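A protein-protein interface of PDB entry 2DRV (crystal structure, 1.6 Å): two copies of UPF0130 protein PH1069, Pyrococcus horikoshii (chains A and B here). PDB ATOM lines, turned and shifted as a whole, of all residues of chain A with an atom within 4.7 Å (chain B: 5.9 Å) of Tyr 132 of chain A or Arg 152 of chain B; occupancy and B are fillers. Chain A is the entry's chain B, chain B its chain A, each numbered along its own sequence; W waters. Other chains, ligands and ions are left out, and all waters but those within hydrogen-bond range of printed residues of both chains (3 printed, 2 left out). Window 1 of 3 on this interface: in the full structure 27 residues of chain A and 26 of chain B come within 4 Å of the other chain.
NH1 of Arg 148 of chain B sits close to OH of Tyr 132 of chain A.
The guanidinium group (NH2) of Arg 152 of chain B lies within hydrogen-bond range of the backbone carbonyl oxygen (O) of Thr 150 of chain A, 2.8 Å away.
O of Arg 152 of chain B sits at hydrogen-bond distance from NH2 of Arg 152 of chain A, 3.3 Å away.
OD1 of Asp 154 of chain B is in salt-bridge range of NE of Arg 152 of chain A, 3.9 Å away.
O of Asp 154 of chain B is in hydrogen-bond range of N of Asp 154 of chain A, at 2.8 Å.
The backbone NH (N) of Val 103 of chain B sits at hydrogen-bond distance from the backbone carbonyl oxygen (O) of Met 153 of chain B.
The guanidinium group (NH1) of Arg 104 of chain B is in hydrogen-bond range of the backbone carbonyl oxygen (O) of Met 153 of chain B (3.4 Å).
The side-chain carboxylate (OD2) of Asp 154 of chain B lies within salt-bridge range of the guanidinium group (NH2) of Arg 104 of chain B, at 3.0 Å.
NH2 of Arg 148 of chain B lies within salt-bridge range of OE2 of Glu 146 of chain B (3.3 Å).
The guanidinium group (NE) of Arg 152 of chain B lies within salt-bridge range of the side-chain carboxylate (OD1) of Asp 154 of chain B (2.9 Å).
The guanidinium group (NH2) of Arg 152 of chain A is in salt-bridge range of the side-chain carboxylate (OD1) of Asp 154 of chain A (3.2 Å).
Phe 66 of chain A touches Arg 152 of chain B.
Tyr 132 of chain A touches Arg 152 of chain B.
Asp 154 of chain A touches Arg 152 of chain B (OD2 to O, 3.8 Å).
OD2 of Asp 154 of chain A touches CA of Met 153 of chain B, at 3.4 Å.
Of chain B, only Arg 148 (3.0 Å) and Arg 152 (3.4 Å) come within 4 Å of Tyr 132 of chain A.
Of chain A, only Phe 66, Tyr 132, Thr 150, Arg 152 and Asp 154 come within 4 Å of Arg 152 of chain B.
Printed residues of chain A within 4 Å of Arg 148 of chain B: Tyr 132.
Printed residues of chain A within 4 Å of Met 153 of chain B: Asp 154.
Of the printed residues of chain B, Arg 152 of chain A touches Arg 152 and Asp 154.
Printed residues of chain B within 4 Å of Asp 154 of chain A: Arg 152, Met 153 and Asp 154.
Arg 104 of chain B touches none of the printed residues of chain A.
The nearest printed residue of chain A that does not touch Arg 152 of chain B is Arg 148 of chain A (4.8 Å).
Of the 12 printed residues of chain A, 5 touch a printed residue of chain B.
Hydrophobic or aromatic side chains of chain A within 4 Å of the printed part of chain B: Phe 66 and Tyr 132.
Among the printed residues, 9 pairs touch across the chains.
Among the printed residues, Asp or Glu carboxylates within 4 Å of a Lys or Arg side-chain nitrogen of the other chain: Arg 152 of chain A with Asp 154 of chain B (3.9 Å).
Thr 150 of chain A touches Arg 152 of chain B, but with the chains exchanged Arg 152 of chain A does not touch Thr 150 of chain B (4.6 Å).
Arg 152 of chain A touches its own counterpart, Arg 152 of chain B.
Arg 152 of chain A touches Asp 154 of chain B, and with the chains exchanged Asp 154 of chain A touches Arg 152 of chain B.
Asp 154 of chain A touches its own counterpart, Asp 154 of chain B.
6 positions are printed for both chains.
Of the 9 pairs that touch across the chains among the printed residues, 4 have their exchanged pair printed and touching as well.
Water W2 bridges ND2 of Asn 134 of chain A and OE1 of Glu 146 of chain B.
Water W1 bridges the backbone carbonyl oxygen (O) of Thr 150 of chain B (2.9 Å) and the guanidinium group (NH1) of Arg 152 of chain A (3.2 Å).
Water W3 lies within hydrogen-bond range of OH of Tyr 132 of chain A (3.4 Å) and NE of Arg 104 of chain B (3.4 Å).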
ATOM      1  N   PHE A  66      -7.320  12.415  -1.337  1.00  0.00           N
ATOM      2  CA  PHE A  66      -6.833  13.754  -1.048  1.00  0.00           C
ATOM      3  C   PHE A  66      -7.898  14.685  -0.451  1.00  0.00           C
ATOM      4  O   PHE A  66      -7.605  15.643   0.252  1.00  0.00           O
ATOM      5  CB  PHE A  66      -6.308  14.364  -2.342  1.00  0.00           C
ATOM      6  CG  PHE A  66      -5.790  15.741  -2.070  1.00  0.00           C
ATOM      7  CD1 PHE A  66      -4.755  15.915  -1.163  1.00  0.00           C
ATOM      8  CD2 PHE A  66      -6.371  16.838  -2.691  1.00  0.00           C
ATOM      9  CE1 PHE A  66      -4.294  17.191  -0.877  1.00  0.00           C
ATOM     10  CE2 PHE A  66      -5.897  18.121  -2.398  1.00  0.00           C
ATOM     11  CZ  PHE A  66      -4.856  18.302  -1.491  1.00  0.00           C
ATOM     12  N   PHE A 130      -1.866  38.430   4.469  1.00  0.00           N
ATOM     13  CA  PHE A 130      -2.891  37.394   4.559  1.00  0.00           C
ATOM     14  C   PHE A 130      -3.934  37.725   3.501  1.00  0.00           C
ATOM     15  O   PHE A 130      -5.001  38.267   3.800  1.00  0.00           O
ATOM     16  CB  PHE A 130      -3.521  37.365   5.958  1.00  0.00           C
ATOM     17  CG  PHE A 130      -2.565  36.974   7.049  1.00  0.00           C
ATOM     18  CD1 PHE A 130      -2.399  35.635   7.398  1.00  0.00           C
ATOM     19  CD2 PHE A 130      -1.833  37.940   7.735  1.00  0.00           C
ATOM     20  CE1 PHE A 130      -1.519  35.257   8.419  1.00  0.00           C
ATOM     21  CE2 PHE A 130      -0.949  37.577   8.760  1.00  0.00           C
ATOM     22  CZ  PHE A 130      -0.793  36.228   9.103  1.00  0.00           C
ATOM     23  N   LYS A 131      -3.608  37.394   2.256  1.00  0.00           N
ATOM     24  CA  LYS A 131      -4.478  37.690   1.120  1.00  0.00           C
ATOM     25  C   LYS A 131      -5.825  36.991   1.099  1.00  0.00           C
ATOM     26  O   LYS A 131      -6.758  37.466   0.448  1.00  0.00           O
ATOM     27  CB  LYS A 131      -3.731  37.416  -0.188  1.00  0.00           C
ATOM     28  CG  LYS A 131      -2.731  38.503  -0.552  1.00  0.00           C
ATOM     29  CD  LYS A 131      -3.442  39.805  -0.918  1.00  0.00           C
ATOM     30  CE  LYS A 131      -2.450  40.915  -1.241  1.00  0.00           C
ATOM     31  NZ  LYS A 131      -3.119  42.214  -1.550  1.00  0.00           N
ATOM     32  N   TYR A 132      -5.940  35.866   1.794  1.00  0.00           N
ATOM     33  CA  TYR A 132      -7.206  35.149   1.830  1.00  0.00           C
ATOM     34  C   TYR A 132      -8.034  35.523   3.046  1.00  0.00           C
ATOM     35  O   TYR A 132      -8.731  34.682   3.611  1.00  0.00           O
ATOM     36  CB  TYR A 132      -6.994  33.633   1.815  1.00  0.00           C
ATOM     37  CG  TYR A 132      -6.565  33.073   0.481  1.00  0.00           C
ATOM     38  CD1 TYR A 132      -7.019  33.636  -0.712  1.00  0.00           C
ATOM     39  CD2 TYR A 132      -5.747  31.947   0.410  1.00  0.00           C
ATOM     40  CE1 TYR A 132      -6.668  33.089  -1.947  1.00  0.00           C
ATOM     41  CE2 TYR A 132      -5.393  31.390  -0.819  1.00  0.00           C
ATOM     42  CZ  TYR A 132      -5.855  31.966  -1.992  1.00  0.00           C
ATOM     43  OH  TYR A 132      -5.513  31.421  -3.210  1.00  0.00           O
ATOM     44  N   SER A 133      -7.950  36.781   3.463  1.00  0.00           N
ATOM     45  CA  SER A 133      -8.759  37.188   4.578  1.00  0.00           C
ATOM     46  C   SER A 133     -10.054  37.753   4.054  1.00  0.00           C
ATOM     47  O   SER A 133     -10.115  38.318   2.973  1.00  0.00           O
ATOM     48  CB  SER A 133      -8.002  38.266   5.351  1.00  0.00           C
ATOM     49  OG  SER A 133      -6.740  37.749   5.757  1.00  0.00           O
ATOM     50  N   ASN A 134     -11.083  37.511   4.835  1.00  0.00           N
ATOM     51  CA  ASN A 134     -12.381  37.965   4.367  1.00  0.00           C
ATOM     52  C   ASN A 134     -13.424  37.844   5.472  1.00  0.00           C
ATOM     53  O   ASN A 134     -13.113  37.611   6.632  1.00  0.00           O
ATOM     54  CB  ASN A 134     -12.786  37.103   3.171  1.00  0.00           C
ATOM     55  CG  ASN A 134     -12.613  35.647   3.520  1.00  0.00           C
ATOM     56  OD1 ASN A 134     -13.165  35.144   4.495  1.00  0.00           O
ATOM     57  ND2 ASN A 134     -11.818  34.954   2.688  1.00  0.00           N
ATOM     58  N   GLU A 146     -12.233  36.012   8.773  1.00  0.00           N
ATOM     59  CA  GLU A 146     -11.253  34.940   8.718  1.00  0.00           C
ATOM     60  C   GLU A 146      -9.974  35.510   8.133  1.00  0.00           C
ATOM     61  O   GLU A 146     -10.004  36.204   7.122  1.00  0.00           O
ATOM     62  CB  GLU A 146     -11.767  33.788   7.855  1.00  0.00           C
ATOM     63  CG  GLU A 146     -10.803  32.622   7.749  1.00  0.00           C
ATOM     64  CD  GLU A 146     -11.441  31.415   7.101  1.00  0.00           C
ATOM     65  OE1 GLU A 146     -11.662  31.447   5.872  1.00  0.00           O
ATOM     66  OE2 GLU A 146     -11.728  30.438   7.822  1.00  0.00           O
ATOM     67  N   ARG A 148      -6.300  34.468   6.700  1.00  0.00           N
ATOM     68  CA  ARG A 148      -5.555  33.318   6.188  1.00  0.00           C
ATOM     69  C   ARG A 148      -4.632  33.740   5.054  1.00  0.00           C
ATOM     70  O   ARG A 148      -4.904  34.716   4.356  1.00  0.00           O
ATOM     71  CB  ARG A 148      -6.558  32.263   5.704  1.00  0.00           C
ATOM     72  CG  ARG A 148      -5.971  30.929   5.270  1.00  0.00           C
ATOM     73  CD  ARG A 148      -7.077  29.885   5.114  1.00  0.00           C
ATOM     74  NE  ARG A 148      -8.029  30.204   4.052  1.00  0.00           N
ATOM     75  CZ  ARG A 148      -7.839  29.940   2.761  1.00  0.00           C
ATOM     76  NH1 ARG A 148      -6.725  29.344   2.357  1.00  0.00           N
ATOM     77  NH2 ARG A 148      -8.769  30.264   1.872  1.00  0.00           N
ATOM     78  N   SER A 149      -3.538  33.000   4.876  1.00  0.00           N
ATOM     79  CA  SER A 149      -2.570  33.303   3.829  1.00  0.00           C
ATOM     80  C   SER A 149      -2.708  32.298   2.687  1.00  0.00           C
ATOM     81  O   SER A 149      -3.361  31.263   2.838  1.00  0.00           O
ATOM     82  CB  SER A 149      -1.149  33.275   4.402  1.00  0.00           C
ATOM     83  OG  SER A 149      -0.229  33.895   3.518  1.00  0.00           O
ATOM     84  N   THR A 150      -2.080  32.597   1.553  1.00  0.00           N
ATOM     85  CA  THR A 150      -2.171  31.740   0.367  1.00  0.00           C
ATOM     86  C   THR A 150      -1.184  30.581   0.251  1.00  0.00           C
ATOM     87  O   THR A 150      -1.463  29.604  -0.445  1.00  0.00           O
ATOM     88  CB  THR A 150      -2.029  32.576  -0.916  1.00  0.00           C
ATOM     89  OG1 THR A 150      -0.724  33.169  -0.949  1.00  0.00           O
ATOM     90  CG2 THR A 150      -3.075  33.676  -0.954  1.00  0.00           C
ATOM     91  N   ARG A 152       0.875  27.204   0.650  1.00  0.00           N
ATOM     92  CA  ARG A 152       0.508  25.852   1.050  1.00  0.00           C
ATOM     93  C   ARG A 152       1.232  24.842   0.177  1.00  0.00           C
ATOM     94  O   ARG A 152       1.800  25.194  -0.859  1.00  0.00           O
ATOM     95  CB  ARG A 152      -0.997  25.633   0.914  1.00  0.00           C
ATOM     96  CG  ARG A 152      -1.509  25.723  -0.508  1.00  0.00           C
ATOM     97  CD  ARG A 152      -3.008  25.467  -0.554  1.00  0.00           C
ATOM     98  NE  ARG A 152      -3.358  24.073  -0.301  1.00  0.00           N
ATOM     99  CZ  ARG A 152      -4.579  23.662   0.032  1.00  0.00           C
ATOM    100  NH1 ARG A 152      -5.561  24.541   0.159  1.00  0.00           N
ATOM    101  NH2 ARG A 152      -4.824  22.374   0.221  1.00  0.00           N
ATOM    102  N   ASP A 154       1.013  20.411  -0.939  1.00  0.00           N
ATOM    103  CA  ASP A 154       0.335  19.125  -0.903  1.00  0.00           C
ATOM    104  C   ASP A 154       1.197  18.181  -1.716  1.00  0.00           C
ATOM    105  O   ASP A 154       1.147  18.184  -2.945  1.00  0.00           O
ATOM    106  CB  ASP A 154      -1.050  19.202  -1.546  1.00  0.00           C
ATOM    107  CG  ASP A 154      -1.880  20.340  -1.007  1.00  0.00           C
ATOM    108  OD1 ASP A 154      -2.436  20.194   0.099  1.00  0.00           O
ATOM    109  OD2 ASP A 154      -1.968  21.379  -1.688  1.00  0.00           O
ATOM    110  N   VAL B 103      -3.734  22.667  -8.713  1.00  0.00           N
ATOM    111  CA  VAL B 103      -5.132  22.355  -8.963  1.00  0.00           C
ATOM    112  C   VAL B 103      -5.868  23.466  -8.234  1.00  0.00           C
ATOM    113  O   VAL B 103      -5.615  23.716  -7.061  1.00  0.00           O
ATOM    114  CB  VAL B 103      -5.548  20.998  -8.367  1.00  0.00           C
ATOM    115  CG1 VAL B 103      -7.032  20.750  -8.623  1.00  0.00           C
ATOM    116  CG2 VAL B 103      -4.717  19.886  -8.993  1.00  0.00           C
ATOM    117  N   ARG B 104      -6.757  24.143  -8.945  1.00  0.00           N
ATOM    118  CA  ARG B 104      -7.519  25.241  -8.361  1.00  0.00           C
ATOM    119  C   ARG B 104      -9.007  24.976  -8.503  1.00  0.00           C
ATOM    120  O   ARG B 104      -9.461  24.487  -9.529  1.00  0.00           O
ATOM    121  CB  ARG B 104      -7.151  26.553  -9.056  1.00  0.00           C
ATOM    122  CG  ARG B 104      -5.757  27.058  -8.716  1.00  0.00           C
ATOM    123  CD  ARG B 104      -5.690  27.552  -7.277  1.00  0.00           C
ATOM    124  NE  ARG B 104      -4.352  27.990  -6.893  1.00  0.00           N
ATOM    125  CZ  ARG B 104      -3.374  27.178  -6.498  1.00  0.00           C
ATOM    126  NH1 ARG B 104      -3.575  25.867  -6.431  1.00  0.00           N
ATOM    127  NH2 ARG B 104      -2.193  27.683  -6.165  1.00  0.00           N
ATOM    128  N   SER B 105      -9.755  25.288  -7.454  1.00  0.00           N
ATOM    129  CA  SER B 105     -11.199  25.098  -7.453  1.00  0.00           C
ATOM    130  C   SER B 105     -11.873  26.179  -8.280  1.00  0.00           C
ATOM    131  O   SER B 105     -11.279  27.221  -8.564  1.00  0.00           O
ATOM    132  CB  SER B 105     -11.735  25.172  -6.024  1.00  0.00           C
ATOM    133  OG  SER B 105     -13.058  25.694  -6.007  1.00  0.00           O
ATOM    134  N   GLU B 146     -17.751  35.828  -2.777  1.00  0.00           N
ATOM    135  CA  GLU B 146     -16.836  34.929  -3.463  1.00  0.00           C
ATOM    136  C   GLU B 146     -17.249  33.500  -3.146  1.00  0.00           C
ATOM    137  O   GLU B 146     -17.452  33.143  -1.986  1.00  0.00           O
ATOM    138  CB  GLU B 146     -15.394  35.157  -3.010  1.00  0.00           C
ATOM    139  CG  GLU B 146     -14.394  34.297  -3.759  1.00  0.00           C
ATOM    140  CD  GLU B 146     -12.965  34.624  -3.391  1.00  0.00           C
ATOM    141  OE1 GLU B 146     -12.509  34.184  -2.313  1.00  0.00           O
ATOM    142  OE2 GLU B 146     -12.307  35.333  -4.176  1.00  0.00           O
ATOM    143  N   ARG B 148     -16.104  29.629  -3.444  1.00  0.00           N
ATOM    144  CA  ARG B 148     -14.915  28.808  -3.666  1.00  0.00           C
ATOM    145  C   ARG B 148     -14.963  27.527  -2.841  1.00  0.00           C
ATOM    146  O   ARG B 148     -15.471  27.522  -1.718  1.00  0.00           O
ATOM    147  CB  ARG B 148     -13.653  29.601  -3.299  1.00  0.00           C
ATOM    148  CG  ARG B 148     -12.353  28.912  -3.688  1.00  0.00           C
ATOM    149  CD  ARG B 148     -11.123  29.658  -3.184  1.00  0.00           C
ATOM    150  NE  ARG B 148     -11.044  31.027  -3.689  1.00  0.00           N
ATOM    151  CZ  ARG B 148      -9.964  31.797  -3.587  1.00  0.00           C
ATOM    152  NH1 ARG B 148      -8.869  31.331  -3.002  1.00  0.00           N
ATOM    153  NH2 ARG B 148      -9.976  33.031  -4.070  1.00  0.00           N
ATOM    154  N   SER B 149     -14.411  26.452  -3.406  1.00  0.00           N
ATOM    155  CA  SER B 149     -14.384  25.148  -2.753  1.00  0.00           C
ATOM    156  C   SER B 149     -13.047  24.907  -2.044  1.00  0.00           C
ATOM    157  O   SER B 149     -12.224  25.818  -1.934  1.00  0.00           O
ATOM    158  CB  SER B 149     -14.648  24.048  -3.786  1.00  0.00           C
ATOM    159  OG  SER B 149     -15.030  22.835  -3.159  1.00  0.00           O
ATOM    160  N   THR B 150     -12.820  23.677  -1.585  1.00  0.00           N
ATOM    161  CA  THR B 150     -11.597  23.359  -0.847  1.00  0.00           C
ATOM    162  C   THR B 150     -10.574  22.396  -1.458  1.00  0.00           C
ATOM    163  O   THR B 150      -9.458  22.295  -0.953  1.00  0.00           O
ATOM    164  CB  THR B 150     -11.947  22.805   0.547  1.00  0.00           C
ATOM    165  OG1 THR B 150     -12.693  21.590   0.400  1.00  0.00           O
ATOM    166  CG2 THR B 150     -12.776  23.810   1.328  1.00  0.00           C
ATOM    167  N   GLU B 151     -10.931  21.700  -2.532  1.00  0.00           N
ATOM    168  CA  GLU B 151     -10.019  20.727  -3.143  1.00  0.00           C
ATOM    169  C   GLU B 151      -8.817  21.305  -3.901  1.00  0.00           C
ATOM    170  O   GLU B 151      -8.519  20.883  -5.019  1.00  0.00           O
ATOM    171  CB  GLU B 151     -10.797  19.799  -4.080  1.00  0.00           C
ATOM    172  CG  GLU B 151     -11.980  19.082  -3.446  1.00  0.00           C
ATOM    173  CD  GLU B 151     -13.077  20.031  -3.002  1.00  0.00           C
ATOM    174  OE1 GLU B 151     -13.400  20.965  -3.765  1.00  0.00           O
ATOM    175  OE2 GLU B 151     -13.623  19.840  -1.894  1.00  0.00           O
ATOM    176  N   ARG B 152      -8.118  22.253  -3.289  1.00  0.00           N
ATOM    177  CA  ARG B 152      -6.948  22.870  -3.915  1.00  0.00           C
ATOM    178  C   ARG B 152      -5.717  21.972  -3.762  1.00  0.00           C
ATOM    179  O   ARG B 152      -5.614  21.226  -2.792  1.00  0.00           O
ATOM    180  CB  ARG B 152      -6.676  24.227  -3.255  1.00  0.00           C
ATOM    181  CG  ARG B 152      -5.402  24.923  -3.707  1.00  0.00           C
ATOM    182  CD  ARG B 152      -5.160  26.194  -2.894  1.00  0.00           C
ATOM    183  NE  ARG B 152      -3.861  26.797  -3.189  1.00  0.00           N
ATOM    184  CZ  ARG B 152      -3.344  27.829  -2.527  1.00  0.00           C
ATOM    185  NH1 ARG B 152      -4.013  28.382  -1.523  1.00  0.00           N
ATOM    186  NH2 ARG B 152      -2.153  28.305  -2.864  1.00  0.00           N
ATOM    187  N   MET B 153      -4.793  22.035  -4.721  1.00  0.00           N
ATOM    188  CA  MET B 153      -3.562  21.247  -4.637  1.00  0.00           C
ATOM    189  C   MET B 153      -2.355  22.038  -5.138  1.00  0.00           C
ATOM    190  O   MET B 153      -2.415  22.707  -6.167  1.00  0.00           O
ATOM    191  CB  MET B 153      -3.677  19.935  -5.425  1.00  0.00           C
ATOM    192  CG  MET B 153      -2.511  18.967  -5.173  1.00  0.00           C
ATOM    193  SD  MET B 153      -2.664  17.252  -6.081  1.00  0.00           S
ATOM    194  CE  MET B 153      -4.533  17.390  -6.548  1.00  0.00           C
ATOM    195  N   ASP B 154      -1.265  21.969  -4.382  1.00  0.00           N
ATOM    196  CA  ASP B 154      -0.026  22.659  -4.732  1.00  0.00           C
ATOM    197  C   ASP B 154       1.107  21.649  -4.536  1.00  0.00           C
ATOM    198  O   ASP B 154       1.624  21.495  -3.431  1.00  0.00           O
ATOM    199  CB  ASP B 154       0.189  23.864  -3.811  1.00  0.00           C
ATOM    200  CG  ASP B 154      -0.836  24.971  -4.033  1.00  0.00           C
ATOM    201  OD1 ASP B 154      -2.049  24.698  -3.940  1.00  0.00           O
ATOM    202  OD2 ASP B 154      -0.419  26.118  -4.293  1.00  0.00           O
ATOM    203  N   PHE B 184     -15.435  18.810  -8.384  1.00  0.00           N
ATOM    204  CA  PHE B 184     -15.819  20.207  -8.565  1.00  0.00           C
ATOM    205  C   PHE B 184     -17.098  20.283  -9.391  1.00  0.00           C
ATOM    206  O   PHE B 184     -18.039  21.003  -9.046  1.00  0.00           O
ATOM    207  CB  PHE B 184     -14.718  20.995  -9.289  1.00  0.00           C
ATOM    208  CG  PHE B 184     -13.464  21.193  -8.478  1.00  0.00           C
ATOM    209  CD1 PHE B 184     -13.534  21.510  -7.122  1.00  0.00           C
ATOM    210  CD2 PHE B 184     -12.213  21.116  -9.085  1.00  0.00           C
ATOM    211  CE1 PHE B 184     -12.374  21.746  -6.386  1.00  0.00           C
ATOM    212  CE2 PHE B 184     -11.050  21.351  -8.357  1.00  0.00           C
ATOM    213  CZ  PHE B 184     -11.129  21.668  -7.005  1.00  0.00           C
HETATM  214  O   HOH W   1      -8.114  23.048   1.492  1.00  0.00           O
HETATM  215  O   HOH W   2     -10.812  34.679   0.499  1.00  0.00           O
HETATM  216  O   HOH W   3      -3.381  31.112  -5.816  1.00  0.00           O
